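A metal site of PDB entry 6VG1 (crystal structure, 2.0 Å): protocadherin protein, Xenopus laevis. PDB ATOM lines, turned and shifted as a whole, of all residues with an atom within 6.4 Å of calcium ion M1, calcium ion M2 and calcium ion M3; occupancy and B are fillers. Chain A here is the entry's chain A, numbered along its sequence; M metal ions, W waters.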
ATOM      1  N   GLU A   9      24.424  17.225  30.548  1.00  0.00           N
ATOM      2  CA  GLU A   9      24.417  18.423  31.373  1.00  0.00           C
ATOM      3  C   GLU A   9      23.115  19.204  31.197  1.00  0.00           C
ATOM      4  O   GLU A   9      22.419  19.057  30.193  1.00  0.00           O
ATOM      5  CB  GLU A   9      25.619  19.322  31.040  1.00  0.00           C
ATOM      6  CG  GLU A   9      25.569  19.984  29.683  1.00  0.00           C
ATOM      7  CD  GLU A   9      26.571  21.123  29.541  1.00  0.00           C
ATOM      8  OE1 GLU A   9      26.742  21.893  30.520  1.00  0.00           O
ATOM      9  OE2 GLU A   9      27.202  21.258  28.465  1.00  0.00           O
ATOM     10  N   GLU A  10      22.779  20.024  32.193  1.00  0.00           N
ATOM     11  CA  GLU A  10      21.600  20.879  32.156  1.00  0.00           C
ATOM     12  C   GLU A  10      20.328  20.077  31.855  1.00  0.00           C
ATOM     13  O   GLU A  10      19.439  20.544  31.143  1.00  0.00           O
ATOM     14  CB  GLU A  10      21.756  22.009  31.131  1.00  0.00           C
ATOM     15  CG  GLU A  10      23.133  22.622  30.999  1.00  0.00           C
ATOM     16  CD  GLU A  10      23.263  23.974  31.704  1.00  0.00           C
ATOM     17  OE1 GLU A  10      22.438  24.283  32.580  1.00  0.00           O
ATOM     18  OE2 GLU A  10      24.216  24.710  31.364  1.00  0.00           O
ATOM     19  N   ARG A  57      20.758  21.733  39.251  1.00  0.00           N
ATOM     20  CA  ARG A  57      21.238  22.027  37.907  1.00  0.00           C
ATOM     21  C   ARG A  57      22.669  21.547  37.736  1.00  0.00           C
ATOM     22  O   ARG A  57      23.512  21.738  38.623  1.00  0.00           O
ATOM     23  CB  ARG A  57      21.134  23.524  37.668  1.00  0.00           C
ATOM     24  CG  ARG A  57      21.576  24.006  36.309  1.00  0.00           C
ATOM     25  CD  ARG A  57      21.397  25.523  36.247  1.00  0.00           C
ATOM     26  NE  ARG A  57      21.811  26.105  34.976  1.00  0.00           N
ATOM     27  CZ  ARG A  57      23.040  26.524  34.726  1.00  0.00           C
ATOM     28  NH1 ARG A  57      23.990  26.431  35.641  1.00  0.00           N
ATOM     29  NH2 ARG A  57      23.328  27.058  33.544  1.00  0.00           N
ATOM     30  N   ILE A  58      22.945  20.921  36.598  1.00  0.00           N
ATOM     31  CA  ILE A  58      24.271  20.392  36.290  1.00  0.00           C
ATOM     32  C   ILE A  58      24.803  21.116  35.055  1.00  0.00           C
ATOM     33  O   ILE A  58      24.368  20.823  33.938  1.00  0.00           O
ATOM     34  CB  ILE A  58      24.260  18.879  36.059  1.00  0.00           C
ATOM     35  CG1 ILE A  58      23.798  18.141  37.309  1.00  0.00           C
ATOM     36  CG2 ILE A  58      25.645  18.404  35.627  1.00  0.00           C
ATOM     37  CD1 ILE A  58      23.575  16.652  37.087  1.00  0.00           C
ATOM     38  N   ASP A  59      25.744  22.044  35.260  1.00  0.00           N
ATOM     39  CA  ASP A  59      26.353  22.805  34.168  1.00  0.00           C
ATOM     40  C   ASP A  59      27.799  22.363  34.001  1.00  0.00           C
ATOM     41  O   ASP A  59      28.657  22.704  34.820  1.00  0.00           O
ATOM     42  CB  ASP A  59      26.267  24.304  34.452  1.00  0.00           C
ATOM     43  CG  ASP A  59      26.736  25.152  33.272  1.00  0.00           C
ATOM     44  OD1 ASP A  59      27.103  24.578  32.222  1.00  0.00           O
ATOM     45  OD2 ASP A  59      26.729  26.395  33.390  1.00  0.00           O
ATOM     46  N   ARG A  60      28.073  21.636  32.916  1.00  0.00           N
ATOM     47  CA  ARG A  60      29.430  21.126  32.699  1.00  0.00           C
ATOM     48  C   ARG A  60      30.441  22.267  32.642  1.00  0.00           C
ATOM     49  O   ARG A  60      31.505  22.197  33.257  1.00  0.00           O
ATOM     50  CB  ARG A  60      29.488  20.302  31.418  1.00  0.00           C
ATOM     51  CG  ARG A  60      30.668  19.335  31.372  1.00  0.00           C
ATOM     52  CD  ARG A  60      31.153  19.077  29.966  1.00  0.00           C
ATOM     53  NE  ARG A  60      31.446  20.334  29.268  1.00  0.00           N
ATOM     54  CZ  ARG A  60      32.449  21.151  29.577  1.00  0.00           C
ATOM     55  NH1 ARG A  60      33.260  20.846  30.579  1.00  0.00           N
ATOM     56  NH2 ARG A  60      32.636  22.258  28.884  1.00  0.00           N
ATOM     57  N   GLU A  61      30.125  23.323  31.898  1.00  0.00           N
ATOM     58  CA  GLU A  61      31.055  24.433  31.735  1.00  0.00           C
ATOM     59  C   GLU A  61      31.380  25.130  33.058  1.00  0.00           C
ATOM     60  O   GLU A  61      32.358  25.887  33.109  1.00  0.00           O
ATOM     61  CB  GLU A  61      30.489  25.439  30.732  1.00  0.00           C
ATOM     62  CG  GLU A  61      30.611  25.017  29.254  1.00  0.00           C
ATOM     63  CD  GLU A  61      29.505  24.098  28.783  1.00  0.00           C
ATOM     64  OE1 GLU A  61      28.316  24.381  29.042  1.00  0.00           O
ATOM     65  OE2 GLU A  61      29.823  23.081  28.137  1.00  0.00           O
ATOM     66  N   ARG A  62      30.612  24.881  34.122  1.00  0.00           N
ATOM     67  CA  ARG A  62      30.869  25.485  35.420  1.00  0.00           C
ATOM     68  C   ARG A  62      31.659  24.583  36.353  1.00  0.00           C
ATOM     69  O   ARG A  62      32.346  25.086  37.244  1.00  0.00           O
ATOM     70  CB  ARG A  62      29.557  25.876  36.102  1.00  0.00           C
ATOM     71  CG  ARG A  62      29.736  26.419  37.509  1.00  0.00           C
ATOM     72  CD  ARG A  62      28.409  26.885  38.112  1.00  0.00           C
ATOM     73  NE  ARG A  62      27.440  25.792  38.210  1.00  0.00           N
ATOM     74  CZ  ARG A  62      27.405  24.904  39.195  1.00  0.00           C
ATOM     75  NH1 ARG A  62      28.299  24.956  40.171  1.00  0.00           N
ATOM     76  NH2 ARG A  62      26.485  23.952  39.196  1.00  0.00           N
ATOM     77  N   ASP A  95      28.703  16.612  27.220  1.00  0.00           N
ATOM     78  CA  ASP A  95      28.682  18.032  26.898  1.00  0.00           C
ATOM     79  C   ASP A  95      27.555  18.329  25.909  1.00  0.00           C
ATOM     80  O   ASP A  95      27.320  17.569  24.968  1.00  0.00           O
ATOM     81  CB  ASP A  95      30.019  18.475  26.312  1.00  0.00           C
ATOM     82  CG  ASP A  95      30.020  19.933  25.875  1.00  0.00           C
ATOM     83  OD1 ASP A  95      29.043  20.662  26.156  1.00  0.00           O
ATOM     84  OD2 ASP A  95      31.008  20.363  25.240  1.00  0.00           O
ATOM     85  N   ILE A  96      26.879  19.463  26.137  1.00  0.00           N
ATOM     86  CA  ILE A  96      25.855  19.976  25.238  1.00  0.00           C
ATOM     87  C   ILE A  96      26.375  21.267  24.637  1.00  0.00           C
ATOM     88  O   ILE A  96      27.206  21.958  25.238  1.00  0.00           O
ATOM     89  CB  ILE A  96      24.519  20.174  25.970  1.00  0.00           C
ATOM     90  CG1 ILE A  96      23.353  20.112  24.982  1.00  0.00           C
ATOM     91  CG2 ILE A  96      24.486  21.500  26.706  1.00  0.00           C
ATOM     92  CD1 ILE A  96      23.153  18.739  24.354  1.00  0.00           C
ATOM     93  N   ASN A  97      25.877  21.593  23.444  1.00  0.00           N
ATOM     94  CA  ASN A  97      26.376  22.736  22.677  1.00  0.00           C
ATOM     95  C   ASN A  97      25.597  24.014  23.010  1.00  0.00           C
ATOM     96  O   ASN A  97      25.082  24.709  22.136  1.00  0.00           O
ATOM     97  CB  ASN A  97      26.283  22.407  21.196  1.00  0.00           C
ATOM     98  CG  ASN A  97      27.054  23.395  20.333  1.00  0.00           C
ATOM     99  OD1 ASN A  97      28.042  23.986  20.780  1.00  0.00           O
ATOM    100  ND2 ASN A  97      26.599  23.583  19.103  1.00  0.00           N
ATOM    101  N   ASP A  98      25.527  24.318  24.301  1.00  0.00           N
ATOM    102  CA  ASP A  98      24.804  25.486  24.790  1.00  0.00           C
ATOM    103  C   ASP A  98      25.684  26.718  24.887  1.00  0.00           C
ATOM    104  O   ASP A  98      25.319  27.674  25.567  1.00  0.00           O
ATOM    105  CB  ASP A  98      24.176  25.186  26.160  1.00  0.00           C
ATOM    106  CG  ASP A  98      25.170  24.580  27.152  1.00  0.00           C
ATOM    107  OD1 ASP A  98      26.338  24.322  26.777  1.00  0.00           O
ATOM    108  OD2 ASP A  98      24.761  24.350  28.309  1.00  0.00           O
ATOM    109  N   ASN A  99      26.827  26.720  24.205  1.00  0.00           N
ATOM    110  CA  ASN A  99      27.683  27.893  24.159  1.00  0.00           C
ATOM    111  C   ASN A  99      28.194  28.075  22.747  1.00  0.00           C
ATOM    112  O   ASN A  99      28.624  27.107  22.094  1.00  0.00           O
ATOM    113  CB  ASN A  99      28.855  27.783  25.133  1.00  0.00           C
ATOM    114  CG  ASN A  99      28.455  28.101  26.557  1.00  0.00           C
ATOM    115  OD1 ASN A  99      28.016  29.219  26.852  1.00  0.00           O
ATOM    116  ND2 ASN A  99      28.578  27.134  27.448  1.00  0.00           N
ATOM    117  N   SER A 100      28.169  29.336  22.288  1.00  0.00           N
ATOM    118  CA  SER A 100      28.551  29.707  20.954  1.00  0.00           C
ATOM    119  C   SER A 100      29.877  30.439  20.968  1.00  0.00           C
ATOM    120  O   SER A 100      30.223  31.095  21.953  1.00  0.00           O
ATOM    121  CB  SER A 100      27.477  30.601  20.363  1.00  0.00           C
ATOM    122  OG  SER A 100      27.052  31.561  21.331  1.00  0.00           O
ATOM    123  N   PRO A 101      30.621  30.383  19.872  1.00  0.00           N
ATOM    124  CA  PRO A 101      31.888  31.140  19.808  1.00  0.00           C
ATOM    125  C   PRO A 101      31.655  32.615  20.065  1.00  0.00           C
ATOM    126  O   PRO A 101      30.677  33.200  19.602  1.00  0.00           O
ATOM    127  CB  PRO A 101      32.394  30.874  18.390  1.00  0.00           C
ATOM    128  CG  PRO A 101      31.757  29.570  17.988  1.00  0.00           C
ATOM    129  CD  PRO A 101      30.387  29.571  18.660  1.00  0.00           C
ATOM    130  N   ASP A 129      34.922  29.354  22.720  1.00  0.00           N
ATOM    131  CA  ASP A 129      33.691  28.575  22.842  1.00  0.00           C
ATOM    132  C   ASP A 129      33.840  27.726  24.089  1.00  0.00           C
ATOM    133  O   ASP A 129      34.741  26.880  24.154  1.00  0.00           O
ATOM    134  CB  ASP A 129      33.463  27.703  21.609  1.00  0.00           C
ATOM    135  CG  ASP A 129      32.105  27.004  21.619  1.00  0.00           C
ATOM    136  OD1 ASP A 129      31.383  26.984  22.649  1.00  0.00           O
ATOM    137  OD2 ASP A 129      31.768  26.426  20.558  1.00  0.00           O
ATOM    138  N   GLU A 130      32.984  27.957  25.086  1.00  0.00           N
ATOM    139  CA  GLU A 130      33.158  27.321  26.383  1.00  0.00           C
ATOM    140  C   GLU A 130      32.773  25.841  26.387  1.00  0.00           C
ATOM    141  O   GLU A 130      32.930  25.203  27.431  1.00  0.00           O
ATOM    142  CB  GLU A 130      32.348  28.081  27.442  1.00  0.00           C
ATOM    143  CG  GLU A 130      32.902  29.466  27.731  1.00  0.00           C
ATOM    144  CD  GLU A 130      32.273  30.104  28.956  1.00  0.00           C
ATOM    145  OE1 GLU A 130      31.283  29.540  29.474  1.00  0.00           O
ATOM    146  OE2 GLU A 130      32.764  31.164  29.395  1.00  0.00           O
ATOM    147  N   ASP A 131      32.275  25.300  25.283  1.00  0.00           N
ATOM    148  CA  ASP A 131      32.087  23.856  25.172  1.00  0.00           C
ATOM    149  C   ASP A 131      33.431  23.185  24.913  1.00  0.00           C
ATOM    150  O   ASP A 131      34.484  23.845  24.899  1.00  0.00           O
ATOM    151  CB  ASP A 131      31.078  23.559  24.068  1.00  0.00           C
ATOM    152  CG  ASP A 131      29.765  24.311  24.255  1.00  0.00           C
ATOM    153  OD1 ASP A 131      29.279  24.436  25.411  1.00  0.00           O
ATOM    154  OD2 ASP A 131      29.209  24.793  23.233  1.00  0.00           O
ATOM    155  N   VAL A 132      33.422  21.863  24.719  1.00  0.00           N
ATOM    156  CA  VAL A 132      34.648  21.126  24.444  1.00  0.00           C
ATOM    157  C   VAL A 132      34.434  20.231  23.224  1.00  0.00           C
ATOM    158  O   VAL A 132      33.318  20.081  22.728  1.00  0.00           O
ATOM    159  CB  VAL A 132      35.108  20.274  25.661  1.00  0.00           C
ATOM    160  CG1 VAL A 132      35.449  21.160  26.849  1.00  0.00           C
ATOM    161  CG2 VAL A 132      34.037  19.263  26.027  1.00  0.00           C
ATOM    162  N   VAL A 134      34.041  18.575  19.687  1.00  0.00           N
ATOM    163  CA  VAL A 134      33.474  19.127  18.460  1.00  0.00           C
ATOM    164  C   VAL A 134      32.701  20.400  18.755  1.00  0.00           C
ATOM    165  O   VAL A 134      32.623  21.308  17.920  1.00  0.00           O
ATOM    166  CB  VAL A 134      32.587  18.093  17.749  1.00  0.00           C
ATOM    167  CG1 VAL A 134      33.370  16.825  17.473  1.00  0.00           C
ATOM    168  CG2 VAL A 134      31.327  17.819  18.571  1.00  0.00           C
ATOM    169  N   ASN A 135      32.102  20.492  19.946  1.00  0.00           N
ATOM    170  CA  ASN A 135      31.360  21.690  20.327  1.00  0.00           C
ATOM    171  C   ASN A 135      32.260  22.893  20.556  1.00  0.00           C
ATOM    172  O   ASN A 135      31.748  23.983  20.831  1.00  0.00           O
ATOM    173  CB  ASN A 135      30.530  21.418  21.570  1.00  0.00           C
ATOM    174  CG  ASN A 135      29.412  20.432  21.309  1.00  0.00           C
ATOM    175  OD1 ASN A 135      29.164  20.074  20.157  1.00  0.00           O
ATOM    176  ND2 ASN A 135      28.738  20.001  22.365  1.00  0.00           N
ATOM    177  N   SER A 136      33.570  22.721  20.433  1.00  0.00           N
ATOM    178  CA  SER A 136      34.521  23.824  20.528  1.00  0.00           C
ATOM    179  C   SER A 136      34.726  24.438  19.142  1.00  0.00           C
ATOM    180  O   SER A 136      34.216  23.940  18.127  1.00  0.00           O
ATOM    181  CB  SER A 136      35.841  23.347  21.100  1.00  0.00           C
ATOM    182  OG  SER A 136      36.549  22.561  20.144  1.00  0.00           O
ATOM    183  N   ILE A 137      35.497  25.513  19.080  1.00  0.00           N
ATOM    184  CA  ILE A 137      35.743  26.207  17.815  1.00  0.00           C
ATOM    185  C   ILE A 137      36.544  25.293  16.902  1.00  0.00           C
ATOM    186  O   ILE A 137      37.656  24.870  17.240  1.00  0.00           O
ATOM    187  CB  ILE A 137      36.477  27.528  18.057  1.00  0.00           C
ATOM    188  CG1 ILE A 137      35.557  28.491  18.816  1.00  0.00           C
ATOM    189  CG2 ILE A 137      36.922  28.150  16.734  1.00  0.00           C
ATOM    190  CD1 ILE A 137      36.234  29.782  19.266  1.00  0.00           C
ATOM    191  N   ASP A 186      31.737  26.132  15.380  1.00  0.00           N
ATOM    192  CA  ASP A 186      32.032  24.857  16.012  1.00  0.00           C
ATOM    193  C   ASP A 186      31.416  23.702  15.219  1.00  0.00           C
ATOM    194  O   ASP A 186      30.727  23.895  14.212  1.00  0.00           O
ATOM    195  CB  ASP A 186      31.526  24.857  17.464  1.00  0.00           C
ATOM    196  CG  ASP A 186      30.007  25.081  17.573  1.00  0.00           C
ATOM    197  OD1 ASP A 186      29.263  24.721  16.629  1.00  0.00           O
ATOM    198  OD2 ASP A 186      29.564  25.616  18.611  1.00  0.00           O
ATOM    199  N   GLY A 187      31.647  22.479  15.715  1.00  0.00           N
ATOM    200  CA  GLY A 187      31.214  21.283  15.025  1.00  0.00           C
ATOM    201  C   GLY A 187      29.808  20.839  15.413  1.00  0.00           C
ATOM    202  O   GLY A 187      29.140  21.444  16.261  1.00  0.00           O
ATOM    203  N   ARG A 192      27.019  26.706  15.792  1.00  0.00           N
ATOM    204  CA  ARG A 192      26.902  28.051  16.333  1.00  0.00           C
ATOM    205  C   ARG A 192      28.110  28.871  15.902  1.00  0.00           C
ATOM    206  O   ARG A 192      29.258  28.446  16.088  1.00  0.00           O
ATOM    207  CB  ARG A 192      26.765  28.019  17.850  1.00  0.00           C
ATOM    208  CG  ARG A 192      25.442  27.384  18.292  1.00  0.00           C
ATOM    209  CD  ARG A 192      25.463  26.895  19.732  1.00  0.00           C
ATOM    210  NE  ARG A 192      25.310  27.959  20.718  1.00  0.00           N
ATOM    211  CZ  ARG A 192      24.199  28.188  21.408  1.00  0.00           C
ATOM    212  NH1 ARG A 192      23.130  27.432  21.229  1.00  0.00           N
ATOM    213  NH2 ARG A 192      24.168  29.176  22.298  1.00  0.00           N
HETATM  214 CA    CA M   1      28.155  22.778  26.816  1.00  0.00          CA
HETATM  215 CA    CA M   2      26.206  24.193  30.024  1.00  0.00          CA
HETATM  216 CA    CA M   3      29.907  25.387  21.113  1.00  0.00          CA
HETATM  217  O   HOH W   1      25.983  27.064  30.602  1.00  0.00           O
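Calcium ion M3 is bound by OD2 of Asp 129 (2.2 Å), OD2 of Asp 131 (2.3 Å), O of Asn 135 (2.3 Å), OD1 of Asn 97 (2.4 Å), O of Asn 99 (2.4 Å), OD2 of Asp 186 (2.5 Å) and OD1 of Asp 129 (2.7 Å).
The backbone NH (N) of Arg 192 sits at hydrogen-bond distance from the side-chain carboxylate (OD1) of Asp 186. O of Asn 97 sits close to NH1 of Arg 192. OD1 of Asp 95 sits close to NE of Arg 60, 3.9 Å away. N of Glu 10 lies within hydrogen-bond range of O of Ile 58 (2.5 Å). The side-chain carboxylate of Asp 59 is in salt-bridge range of the guanidinium group of Arg 57, at 3.5 Å. OE1 of Glu 61 sits close to ND2 of Asn 99 (3.2 Å). The guanidinium group (NH2) of Arg 57 is in salt-bridge range of the side-chain carboxylate (OE1) of Glu 10 (3.1 Å). N of Arg 60 sits close to OE1 of Glu 9 (2.8 Å).
Six residues have an atom within 4 Å of calcium ion M3: Asn 97, Asn 99, Asp 129, Asp 131, Asn 135 and Asp 186. The nearest printed residue that does not touch calcium ion M3 is Ser 100 (4.5 Å).
Of the 26 residues printed, 6 come within 4 Å of calcium ion M1.
Calcium ion M2 is bound by the side-chain carboxylate (OD2) of Asp 98 (2.2 Å). OE1 of Glu 61 binds calcium ion M2. OD1 of Asp 59 is bound to calcium ion M2, at 2.4 Å. Calcium ion M2 is bound by OE1 of Glu 9, 2.4 Å away. Calcium ion M2 is bound by OE2 of Glu 10 (2.5 Å). Calcium ion M2 has five donor atoms within binding distance. Slightly farther from calcium ion M2 lies water W1 (2.9 Å).
The backbone carbonyl oxygen (O) of Ile 96 binds calcium ion M1. Calcium ion M1 is bound by the side-chain carboxylate (OE2) of Glu 61 (2.1 Å). The side-chain carboxylate (OD1) of Asp 98 binds calcium ion M1. OD1 of Asp 95 binds calcium ion M1 (2.4 Å). Calcium ion M1 is bound by the side-chain carboxylate (OE2) of Glu 9, at 2.4 Å. Calcium ion M1 is bound by OD1 of Asp 131 (2.4 Å). Calcium ion M1 is bound by OE1 of Glu 61 (2.7 Å).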
